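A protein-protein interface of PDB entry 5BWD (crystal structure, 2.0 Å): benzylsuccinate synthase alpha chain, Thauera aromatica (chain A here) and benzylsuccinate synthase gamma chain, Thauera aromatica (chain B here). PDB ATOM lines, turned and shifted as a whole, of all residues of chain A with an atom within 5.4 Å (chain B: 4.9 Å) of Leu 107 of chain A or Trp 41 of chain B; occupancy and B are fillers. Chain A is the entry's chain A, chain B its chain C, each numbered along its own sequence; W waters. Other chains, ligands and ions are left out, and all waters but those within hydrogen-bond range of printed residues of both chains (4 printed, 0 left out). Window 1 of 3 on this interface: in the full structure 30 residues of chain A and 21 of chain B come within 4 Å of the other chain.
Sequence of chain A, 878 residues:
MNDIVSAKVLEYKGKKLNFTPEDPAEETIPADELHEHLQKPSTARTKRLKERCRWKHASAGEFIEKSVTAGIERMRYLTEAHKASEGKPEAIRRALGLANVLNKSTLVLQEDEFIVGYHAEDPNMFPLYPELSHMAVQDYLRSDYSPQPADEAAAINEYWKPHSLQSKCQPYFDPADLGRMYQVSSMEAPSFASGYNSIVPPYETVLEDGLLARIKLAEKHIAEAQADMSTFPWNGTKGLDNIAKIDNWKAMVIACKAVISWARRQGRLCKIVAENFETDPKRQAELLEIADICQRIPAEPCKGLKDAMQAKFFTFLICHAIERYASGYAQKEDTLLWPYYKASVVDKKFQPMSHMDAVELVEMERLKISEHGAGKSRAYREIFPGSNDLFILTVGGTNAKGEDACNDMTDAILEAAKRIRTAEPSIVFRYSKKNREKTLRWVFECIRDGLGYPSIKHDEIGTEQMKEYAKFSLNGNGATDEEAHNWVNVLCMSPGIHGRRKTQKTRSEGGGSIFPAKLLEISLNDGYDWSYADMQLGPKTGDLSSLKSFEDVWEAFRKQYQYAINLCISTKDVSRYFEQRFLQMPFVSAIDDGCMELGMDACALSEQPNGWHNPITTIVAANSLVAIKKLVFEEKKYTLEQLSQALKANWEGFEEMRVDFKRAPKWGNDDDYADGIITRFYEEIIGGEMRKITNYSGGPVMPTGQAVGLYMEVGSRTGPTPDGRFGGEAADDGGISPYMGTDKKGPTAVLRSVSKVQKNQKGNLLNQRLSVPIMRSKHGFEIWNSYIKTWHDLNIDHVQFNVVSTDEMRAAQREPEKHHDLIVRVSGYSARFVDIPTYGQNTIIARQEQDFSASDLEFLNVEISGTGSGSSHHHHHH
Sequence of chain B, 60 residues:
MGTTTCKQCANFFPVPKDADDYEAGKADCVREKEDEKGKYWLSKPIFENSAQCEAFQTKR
The backbone carbonyl oxygen of Leu 109 of chain A lies within hydrogen-bond range of the backbone NH of Trp 41 of chain B, at 2.7 Å. N of Leu 107 of chain A lies within hydrogen-bond range of O of Ser 43 of chain B (2.9 Å). OE2 of Glu 111 of chain A sits at hydrogen-bond distance from N of Lys 39 of chain B.
Water W1 lies within hydrogen-bond range of OG of Ser 43 of chain B (2.7 Å) and NH2 of Arg 265 of chain A (2.9 Å). Water W4 lies within hydrogen-bond range of O of Lys 39 of chain B (2.8 Å) and OE1 of Gln 110 of chain A (3.0 Å). Water W2 lies within hydrogen-bond range of OG of Ser 43 of chain B (3.0 Å), O of Arg 265 of chain A (3.0 Å) and N of Leu 269 of chain A (3.4 Å). Water W3 lies within hydrogen-bond range of the side-chain carboxylate (OE2) of Glu 32 of chain B (3.0 Å), the side-chain amino group (NZ) of Lys 39 of chain B (3.1 Å) and the backbone carbonyl oxygen (O) of Phe 277 of chain A (3.1 Å).
Of the printed residues of chain B, Gln 110 of chain A touches Lys 39, Tyr 40 and Trp 41. Printed residues of chain B within 4 Å of Leu 269 of chain A: Val 30 and Ser 43. Of the printed residues of chain A, Glu 32 of chain B touches Phe 277 (3.7 Å). Of the printed residues of chain A, Trp 41 of chain B touches Leu 107, Val 108, Leu 109, Gln 110, Glu 111, Val 273, Phe 277 and Glu 278. Of the printed residues of chain A, Leu 42 of chain B touches Thr 106, Leu 107 and Val 108.
Among the printed residues, pairs that only touch across the chains: Leu 109 of chain A with Tyr 40 of chain B (3.2 Å), Thr 106 of chain A with Ser 43 of chain B (3.3 Å), Leu 107 of chain A with Leu 42 of chain B (3.4 Å), Phe 277 of chain A with Trp 41 of chain B (3.4 Å), Val 108 of chain A with Trp 41 of chain B (3.5 Å), Val 273 of chain A with Trp 41 of chain B (3.6 Å), Leu 107 of chain A with Trp 41 of chain B (3.6 Å), Arg 265 of chain A with Ser 43 of chain B (3.7 Å), Val 108 of chain A with Leu 42 of chain B (3.7 Å), Phe 277 of chain A with Glu 32 of chain B (3.7 Å), Leu 269 of chain A with Ser 43 of chain B (3.8 Å), Thr 106 of chain A with Leu 42 of chain B (3.8 Å), Gln 110 of chain A with Lys 39 of chain B (3.8 Å), Glu 278 of chain A with Trp 41 of chain B (3.8 Å), Phe 277 of chain A with Val 30 of chain B (3.8 Å), Gln 110 of chain A with Tyr 40 of chain B (3.8 Å), Glu 111 of chain A with Trp 41 of chain B (3.9 Å), Ser 105 of chain A with Ser 43 of chain B (3.9 Å), Leu 269 of chain A with Val 30 of chain B (3.9 Å) and Gln 110 of chain A with Trp 41 of chain B (3.9 Å).
NE1 of Trp 41 of chain B is in hydrogen-bond range of OE2 of Glu 32 of chain B. O of Ser 105 of chain A sits at hydrogen-bond distance from NH1 of Arg 265 of chain A, 2.8 Å away. O of Arg 31 of chain B sits at hydrogen-bond distance from N of Leu 42 of chain B. O of Val 273 of chain A is in hydrogen-bond range of N of Glu 278 of chain A (2.7 Å). The side-chain carboxylate (OE1) of Glu 32 of chain B is in salt-bridge range of the side-chain amino group (NZ) of Lys 39 of chain B. The backbone carbonyl oxygen (O) of Leu 102 of chain A sits at hydrogen-bond distance from the guanidinium group (NH1) of Arg 265 of chain A (2.8 Å).
Of the 8 printed residues of chain B, 7 touch a printed residue of chain A. Hydrophobic or aromatic side chains of chain B within 4 Å of the printed part of chain A: Val 30, Tyr 40, Trp 41 and Leu 42. Of the 15 printed residues of chain A, 12 touch a printed residue of chain B. Hydrophobic or aromatic side chains of chain A that line the printed part of chain B: Val 108, Leu 269, Val 273 and Phe 277. Among the printed residues, no Asp or Glu carboxylate lies within 4 Å of a Lys or Arg side-chain nitrogen of the other chain.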
ATOM      1  N   LEU A 102      22.382  35.238   7.367  1.00  0.00           N
ATOM      2  CA  LEU A 102      21.733  34.961   6.089  1.00  0.00           C
ATOM      3  C   LEU A 102      22.675  35.154   4.902  1.00  0.00           C
ATOM      4  O   LEU A 102      22.636  34.378   3.947  1.00  0.00           O
ATOM      5  CB  LEU A 102      20.494  35.847   5.920  1.00  0.00           C
ATOM      6  CG  LEU A 102      19.315  35.573   6.855  1.00  0.00           C
ATOM      7  CD1 LEU A 102      18.207  36.604   6.643  1.00  0.00           C
ATOM      8  CD2 LEU A 102      18.779  34.165   6.652  1.00  0.00           C
ATOM      9  N   SER A 105      25.563  32.152   5.351  1.00  0.00           N
ATOM     10  CA  SER A 105      25.139  30.767   5.556  1.00  0.00           C
ATOM     11  C   SER A 105      25.284  29.918   4.299  1.00  0.00           C
ATOM     12  O   SER A 105      24.939  30.350   3.197  1.00  0.00           O
ATOM     13  CB  SER A 105      23.679  30.698   6.025  1.00  0.00           C
ATOM     14  OG  SER A 105      23.564  30.972   7.411  1.00  0.00           O
ATOM     15  N   THR A 106      25.800  28.708   4.479  1.00  0.00           N
ATOM     16  CA  THR A 106      25.744  27.690   3.443  1.00  0.00           C
ATOM     17  C   THR A 106      24.279  27.324   3.232  1.00  0.00           C
ATOM     18  O   THR A 106      23.570  27.053   4.200  1.00  0.00           O
ATOM     19  CB  THR A 106      26.551  26.436   3.831  1.00  0.00           C
ATOM     20  OG1 THR A 106      27.924  26.789   4.037  1.00  0.00           O
ATOM     21  CG2 THR A 106      26.449  25.370   2.748  1.00  0.00           C
ATOM     22  N   LEU A 107      23.824  27.336   1.979  1.00  0.00           N
ATOM     23  CA  LEU A 107      22.427  27.023   1.667  1.00  0.00           C
ATOM     24  C   LEU A 107      22.297  25.590   1.159  1.00  0.00           C
ATOM     25  O   LEU A 107      23.254  25.030   0.623  1.00  0.00           O
ATOM     26  CB  LEU A 107      21.864  28.002   0.631  1.00  0.00           C
ATOM     27  CG  LEU A 107      21.954  29.492   0.977  1.00  0.00           C
ATOM     28  CD1 LEU A 107      21.207  30.326  -0.051  1.00  0.00           C
ATOM     29  CD2 LEU A 107      21.437  29.764   2.383  1.00  0.00           C
ATOM     30  N   VAL A 108      21.111  25.008   1.322  1.00  0.00           N
ATOM     31  CA  VAL A 108      20.895  23.600   1.007  1.00  0.00           C
ATOM     32  C   VAL A 108      19.801  23.402  -0.040  1.00  0.00           C
ATOM     33  O   VAL A 108      18.747  24.033   0.018  1.00  0.00           O
ATOM     34  CB  VAL A 108      20.550  22.795   2.280  1.00  0.00           C
ATOM     35  CG1 VAL A 108      20.448  21.305   1.958  1.00  0.00           C
ATOM     36  CG2 VAL A 108      21.583  23.042   3.373  1.00  0.00           C
ATOM     37  N   LEU A 109      20.072  22.519  -0.996  1.00  0.00           N
ATOM     38  CA  LEU A 109      19.074  22.059  -1.954  1.00  0.00           C
ATOM     39  C   LEU A 109      19.139  20.540  -2.036  1.00  0.00           C
ATOM     40  O   LEU A 109      20.224  19.974  -2.149  1.00  0.00           O
ATOM     41  CB  LEU A 109      19.304  22.672  -3.336  1.00  0.00           C
ATOM     42  CG  LEU A 109      18.476  22.038  -4.460  1.00  0.00           C
ATOM     43  CD1 LEU A 109      16.994  22.354  -4.286  1.00  0.00           C
ATOM     44  CD2 LEU A 109      18.968  22.480  -5.829  1.00  0.00           C
ATOM     45  N   GLN A 110      17.987  19.879  -1.975  1.00  0.00           N
ATOM     46  CA  GLN A 110      17.950  18.419  -2.009  1.00  0.00           C
ATOM     47  C   GLN A 110      17.228  17.898  -3.247  1.00  0.00           C
ATOM     48  O   GLN A 110      16.491  18.633  -3.907  1.00  0.00           O
ATOM     49  CB  GLN A 110      17.270  17.867  -0.754  1.00  0.00           C
ATOM     50  CG  GLN A 110      17.884  18.326   0.556  1.00  0.00           C
ATOM     51  CD  GLN A 110      17.386  17.519   1.739  1.00  0.00           C
ATOM     52  OE1 GLN A 110      17.360  16.286   1.695  1.00  0.00           O
ATOM     53  NE2 GLN A 110      16.987  18.208   2.804  1.00  0.00           N
ATOM     54  N   GLU A 111      17.437  16.625  -3.561  1.00  0.00           N
ATOM     55  CA  GLU A 111      16.705  16.005  -4.658  1.00  0.00           C
ATOM     56  C   GLU A 111      15.227  15.890  -4.299  1.00  0.00           C
ATOM     57  O   GLU A 111      14.878  15.796  -3.121  1.00  0.00           O
ATOM     58  CB  GLU A 111      17.284  14.629  -4.994  1.00  0.00           C
ATOM     59  CG  GLU A 111      17.285  13.642  -3.836  1.00  0.00           C
ATOM     60  CD  GLU A 111      17.741  12.257  -4.258  1.00  0.00           C
ATOM     61  OE1 GLU A 111      17.343  11.809  -5.353  1.00  0.00           O
ATOM     62  OE2 GLU A 111      18.506  11.619  -3.503  1.00  0.00           O
ATOM     63  N   TRP A 262      18.865  36.375   0.665  1.00  0.00           N
ATOM     64  CA  TRP A 262      18.948  34.972   1.060  1.00  0.00           C
ATOM     65  C   TRP A 262      18.055  34.084   0.187  1.00  0.00           C
ATOM     66  O   TRP A 262      18.488  33.036  -0.313  1.00  0.00           O
ATOM     67  CB  TRP A 262      18.572  34.876   2.540  1.00  0.00           C
ATOM     68  CG  TRP A 262      18.404  33.521   3.150  1.00  0.00           C
ATOM     69  CD1 TRP A 262      19.386  32.621   3.445  1.00  0.00           C
ATOM     70  CD2 TRP A 262      17.180  32.953   3.630  1.00  0.00           C
ATOM     71  NE1 TRP A 262      18.841  31.509   4.048  1.00  0.00           N
ATOM     72  CE2 TRP A 262      17.489  31.691   4.173  1.00  0.00           C
ATOM     73  CE3 TRP A 262      15.850  33.384   3.639  1.00  0.00           C
ATOM     74  CZ2 TRP A 262      16.516  30.855   4.716  1.00  0.00           C
ATOM     75  CZ3 TRP A 262      14.884  32.552   4.180  1.00  0.00           C
ATOM     76  CH2 TRP A 262      15.223  31.303   4.710  1.00  0.00           C
ATOM     77  N   ARG A 265      19.487  33.973  -3.315  1.00  0.00           N
ATOM     78  CA  ARG A 265      20.696  33.158  -3.381  1.00  0.00           C
ATOM     79  C   ARG A 265      20.310  31.679  -3.372  1.00  0.00           C
ATOM     80  O   ARG A 265      20.974  30.849  -3.995  1.00  0.00           O
ATOM     81  CB  ARG A 265      21.647  33.488  -2.224  1.00  0.00           C
ATOM     82  CG  ARG A 265      23.019  32.830  -2.343  1.00  0.00           C
ATOM     83  CD  ARG A 265      24.062  33.519  -1.463  1.00  0.00           C
ATOM     84  NE  ARG A 265      23.695  33.503  -0.051  1.00  0.00           N
ATOM     85  CZ  ARG A 265      24.027  32.533   0.794  1.00  0.00           C
ATOM     86  NH1 ARG A 265      23.649  32.598   2.064  1.00  0.00           N
ATOM     87  NH2 ARG A 265      24.737  31.497   0.368  1.00  0.00           N
ATOM     88  N   GLN A 266      19.226  31.363  -2.667  1.00  0.00           N
ATOM     89  CA  GLN A 266      18.646  30.020  -2.684  1.00  0.00           C
ATOM     90  C   GLN A 266      18.173  29.669  -4.089  1.00  0.00           C
ATOM     91  O   GLN A 266      18.361  28.547  -4.560  1.00  0.00           O
ATOM     92  CB  GLN A 266      17.478  29.919  -1.698  1.00  0.00           C
ATOM     93  CG  GLN A 266      16.794  28.556  -1.675  1.00  0.00           C
ATOM     94  CD  GLN A 266      17.582  27.518  -0.901  1.00  0.00           C
ATOM     95  OE1 GLN A 266      18.080  27.788   0.193  1.00  0.00           O
ATOM     96  NE2 GLN A 266      17.703  26.321  -1.468  1.00  0.00           N
ATOM     97  N   LEU A 269      21.076  28.870  -6.307  1.00  0.00           N
ATOM     98  CA  LEU A 269      21.523  27.496  -6.096  1.00  0.00           C
ATOM     99  C   LEU A 269      20.723  26.514  -6.958  1.00  0.00           C
ATOM    100  O   LEU A 269      21.292  25.598  -7.552  1.00  0.00           O
ATOM    101  CB  LEU A 269      21.414  27.119  -4.616  1.00  0.00           C
ATOM    102  CG  LEU A 269      21.691  25.655  -4.259  1.00  0.00           C
ATOM    103  CD1 LEU A 269      23.040  25.195  -4.807  1.00  0.00           C
ATOM    104  CD2 LEU A 269      21.627  25.446  -2.753  1.00  0.00           C
ATOM    105  N   VAL A 273      22.356  24.225  -9.999  1.00  0.00           N
ATOM    106  CA  VAL A 273      22.225  22.772  -9.997  1.00  0.00           C
ATOM    107  C   VAL A 273      21.531  22.280 -11.268  1.00  0.00           C
ATOM    108  O   VAL A 273      21.942  21.277 -11.860  1.00  0.00           O
ATOM    109  CB  VAL A 273      21.476  22.288  -8.739  1.00  0.00           C
ATOM    110  CG1 VAL A 273      21.085  20.823  -8.872  1.00  0.00           C
ATOM    111  CG2 VAL A 273      22.336  22.500  -7.504  1.00  0.00           C
ATOM    112  N   PHE A 277      24.575  20.360 -12.535  1.00  0.00           N
ATOM    113  CA  PHE A 277      24.637  19.132 -11.742  1.00  0.00           C
ATOM    114  C   PHE A 277      23.527  18.131 -12.061  1.00  0.00           C
ATOM    115  O   PHE A 277      23.791  16.945 -12.258  1.00  0.00           O
ATOM    116  CB  PHE A 277      24.596  19.468 -10.248  1.00  0.00           C
ATOM    117  CG  PHE A 277      25.806  20.206  -9.755  1.00  0.00           C
ATOM    118  CD1 PHE A 277      25.874  21.588  -9.839  1.00  0.00           C
ATOM    119  CD2 PHE A 277      26.874  19.521  -9.199  1.00  0.00           C
ATOM    120  CE1 PHE A 277      26.985  22.271  -9.384  1.00  0.00           C
ATOM    121  CE2 PHE A 277      27.992  20.197  -8.740  1.00  0.00           C
ATOM    122  CZ  PHE A 277      28.048  21.574  -8.833  1.00  0.00           C
ATOM    123  N   GLU A 278      22.288  18.608 -12.091  1.00  0.00           N
ATOM    124  CA  GLU A 278      21.138  17.734 -12.300  1.00  0.00           C
ATOM    125  C   GLU A 278      21.100  17.183 -13.724  1.00  0.00           C
ATOM    126  O   GLU A 278      21.241  17.934 -14.689  1.00  0.00           O
ATOM    127  CB  GLU A 278      19.840  18.481 -11.992  1.00  0.00           C
ATOM    128  CG  GLU A 278      18.590  17.652 -12.225  1.00  0.00           C
ATOM    129  CD  GLU A 278      18.534  16.427 -11.333  1.00  0.00           C
ATOM    130  OE1 GLU A 278      18.287  15.322 -11.855  1.00  0.00           O
ATOM    131  OE2 GLU A 278      18.733  16.572 -10.108  1.00  0.00           O
ATOM    132  N   VAL B  30      29.704  25.614  -4.814  1.00  0.00           N
ATOM    133  CA  VAL B  30      28.658  24.603  -4.823  1.00  0.00           C
ATOM    134  C   VAL B  30      29.247  23.196  -4.868  1.00  0.00           C
ATOM    135  O   VAL B  30      29.982  22.848  -5.789  1.00  0.00           O
ATOM    136  CB  VAL B  30      27.693  24.827  -5.997  1.00  0.00           C
ATOM    137  CG1 VAL B  30      26.544  23.832  -5.933  1.00  0.00           C
ATOM    138  CG2 VAL B  30      27.163  26.255  -5.978  1.00  0.00           C
ATOM    139  N   ARG B  31      28.917  22.395  -3.860  1.00  0.00           N
ATOM    140  CA  ARG B  31      29.383  21.015  -3.781  1.00  0.00           C
ATOM    141  C   ARG B  31      28.202  20.053  -3.742  1.00  0.00           C
ATOM    142  O   ARG B  31      27.186  20.331  -3.105  1.00  0.00           O
ATOM    143  CB  ARG B  31      30.257  20.807  -2.543  1.00  0.00           C
ATOM    144  CG  ARG B  31      31.435  21.762  -2.433  1.00  0.00           C
ATOM    145  CD  ARG B  31      32.100  21.654  -1.066  1.00  0.00           C
ATOM    146  NE  ARG B  31      32.690  20.337  -0.841  1.00  0.00           N
ATOM    147  CZ  ARG B  31      33.986  20.067  -0.965  1.00  0.00           C
ATOM    148  NH1 ARG B  31      34.435  18.838  -0.742  1.00  0.00           N
ATOM    149  NH2 ARG B  31      34.837  21.026  -1.307  1.00  0.00           N
ATOM    150  N   GLU B  32      28.339  18.922  -4.423  1.00  0.00           N
ATOM    151  CA  GLU B  32      27.323  17.876  -4.379  1.00  0.00           C
ATOM    152  C   GLU B  32      27.705  16.826  -3.345  1.00  0.00           C
ATOM    153  O   GLU B  32      28.864  16.428  -3.253  1.00  0.00           O
ATOM    154  CB  GLU B  32      27.146  17.230  -5.755  1.00  0.00           C
ATOM    155  CG  GLU B  32      26.195  16.044  -5.764  1.00  0.00           C
ATOM    156  CD  GLU B  32      25.991  15.473  -7.150  1.00  0.00           C
ATOM    157  OE1 GLU B  32      26.204  14.254  -7.331  1.00  0.00           O
ATOM    158  OE2 GLU B  32      25.612  16.243  -8.059  1.00  0.00           O
ATOM    159  N   LYS B  39      20.685  12.544  -2.291  1.00  0.00           N
ATOM    160  CA  LYS B  39      21.597  13.540  -2.832  1.00  0.00           C
ATOM    161  C   LYS B  39      21.170  14.957  -2.465  1.00  0.00           C
ATOM    162  O   LYS B  39      19.980  15.248  -2.339  1.00  0.00           O
ATOM    163  CB  LYS B  39      21.684  13.391  -4.352  1.00  0.00           C
ATOM    164  CG  LYS B  39      22.715  14.279  -5.018  1.00  0.00           C
ATOM    165  CD  LYS B  39      22.803  13.989  -6.507  1.00  0.00           C
ATOM    166  CE  LYS B  39      23.235  12.558  -6.770  1.00  0.00           C
ATOM    167  NZ  LYS B  39      23.415  12.303  -8.227  1.00  0.00           N
ATOM    168  N   TYR B  40      22.150  15.836  -2.283  1.00  0.00           N
ATOM    169  CA  TYR B  40      21.863  17.246  -2.055  1.00  0.00           C
ATOM    170  C   TYR B  40      23.051  18.118  -2.433  1.00  0.00           C
ATOM    171  O   TYR B  40      24.153  17.620  -2.659  1.00  0.00           O
ATOM    172  CB  TYR B  40      21.460  17.492  -0.599  1.00  0.00           C
ATOM    173  CG  TYR B  40      22.526  17.198   0.431  1.00  0.00           C
ATOM    174  CD1 TYR B  40      22.693  15.918   0.943  1.00  0.00           C
ATOM    175  CD2 TYR B  40      23.349  18.210   0.917  1.00  0.00           C
ATOM    176  CE1 TYR B  40      23.659  15.648   1.895  1.00  0.00           C
ATOM    177  CE2 TYR B  40      24.318  17.951   1.868  1.00  0.00           C
ATOM    178  CZ  TYR B  40      24.465  16.670   2.355  1.00  0.00           C
ATOM    179  OH  TYR B  40      25.423  16.409   3.305  1.00  0.00           O
ATOM    180  N   TRP B  41      22.818  19.424  -2.503  1.00  0.00           N
ATOM    181  CA  TRP B  41      23.856  20.366  -2.899  1.00  0.00           C
ATOM    182  C   TRP B  41      24.008  21.495  -1.880  1.00  0.00           C
ATOM    183  O   TRP B  41      23.021  21.980  -1.319  1.00  0.00           O
ATOM    184  CB  TRP B  41      23.549  20.934  -4.284  1.00  0.00           C
ATOM    185  CG  TRP B  41      23.495  19.876  -5.349  1.00  0.00           C
ATOM    186  CD1 TRP B  41      24.519  19.476  -6.155  1.00  0.00           C
ATOM    187  CD2 TRP B  41      22.363  19.073  -5.712  1.00  0.00           C
ATOM    188  NE1 TRP B  41      24.097  18.476  -7.002  1.00  0.00           N
ATOM    189  CE2 TRP B  41      22.775  18.213  -6.751  1.00  0.00           C
ATOM    190  CE3 TRP B  41      21.040  19.002  -5.263  1.00  0.00           C
ATOM    191  CZ2 TRP B  41      21.915  17.293  -7.346  1.00  0.00           C
ATOM    192  CZ3 TRP B  41      20.188  18.089  -5.854  1.00  0.00           C
ATOM    193  CH2 TRP B  41      20.628  17.245  -6.887  1.00  0.00           C
ATOM    194  N   LEU B  42      25.251  21.905  -1.651  1.00  0.00           N
ATOM    195  CA  LEU B  42      25.558  22.960  -0.689  1.00  0.00           C
ATOM    196  C   LEU B  42      26.170  24.170  -1.385  1.00  0.00           C
ATOM    197  O   LEU B  42      27.108  24.031  -2.166  1.00  0.00           O
ATOM    198  CB  LEU B  42      26.517  22.445   0.388  1.00  0.00           C
ATOM    199  CG  LEU B  42      26.020  21.319   1.296  1.00  0.00           C
ATOM    200  CD1 LEU B  42      27.104  20.920   2.291  1.00  0.00           C
ATOM    201  CD2 LEU B  42      24.754  21.738   2.024  1.00  0.00           C
ATOM    202  N   SER B  43      25.638  25.353  -1.093  1.00  0.00           N
ATOM    203  CA  SER B  43      26.150  26.591  -1.672  1.00  0.00           C
ATOM    204  C   SER B  43      26.709  27.507  -0.590  1.00  0.00           C
ATOM    205  O   SER B  43      25.963  28.061   0.214  1.00  0.00           O
ATOM    206  CB  SER B  43      25.050  27.314  -2.452  1.00  0.00           C
ATOM    207  OG  SER B  43      25.520  28.543  -2.975  1.00  0.00           O
HETATM  208  O   HOH W   1      26.400  30.796  -1.845  1.00  0.00           O
HETATM  209  O   HOH W   2      23.773  30.141  -4.737  1.00  0.00           O
HETATM  210  O   HOH W   3      23.698  14.832  -9.957  1.00  0.00           O
HETATM  211  O   HOH W   4      18.864  14.361   0.038  1.00  0.00           O
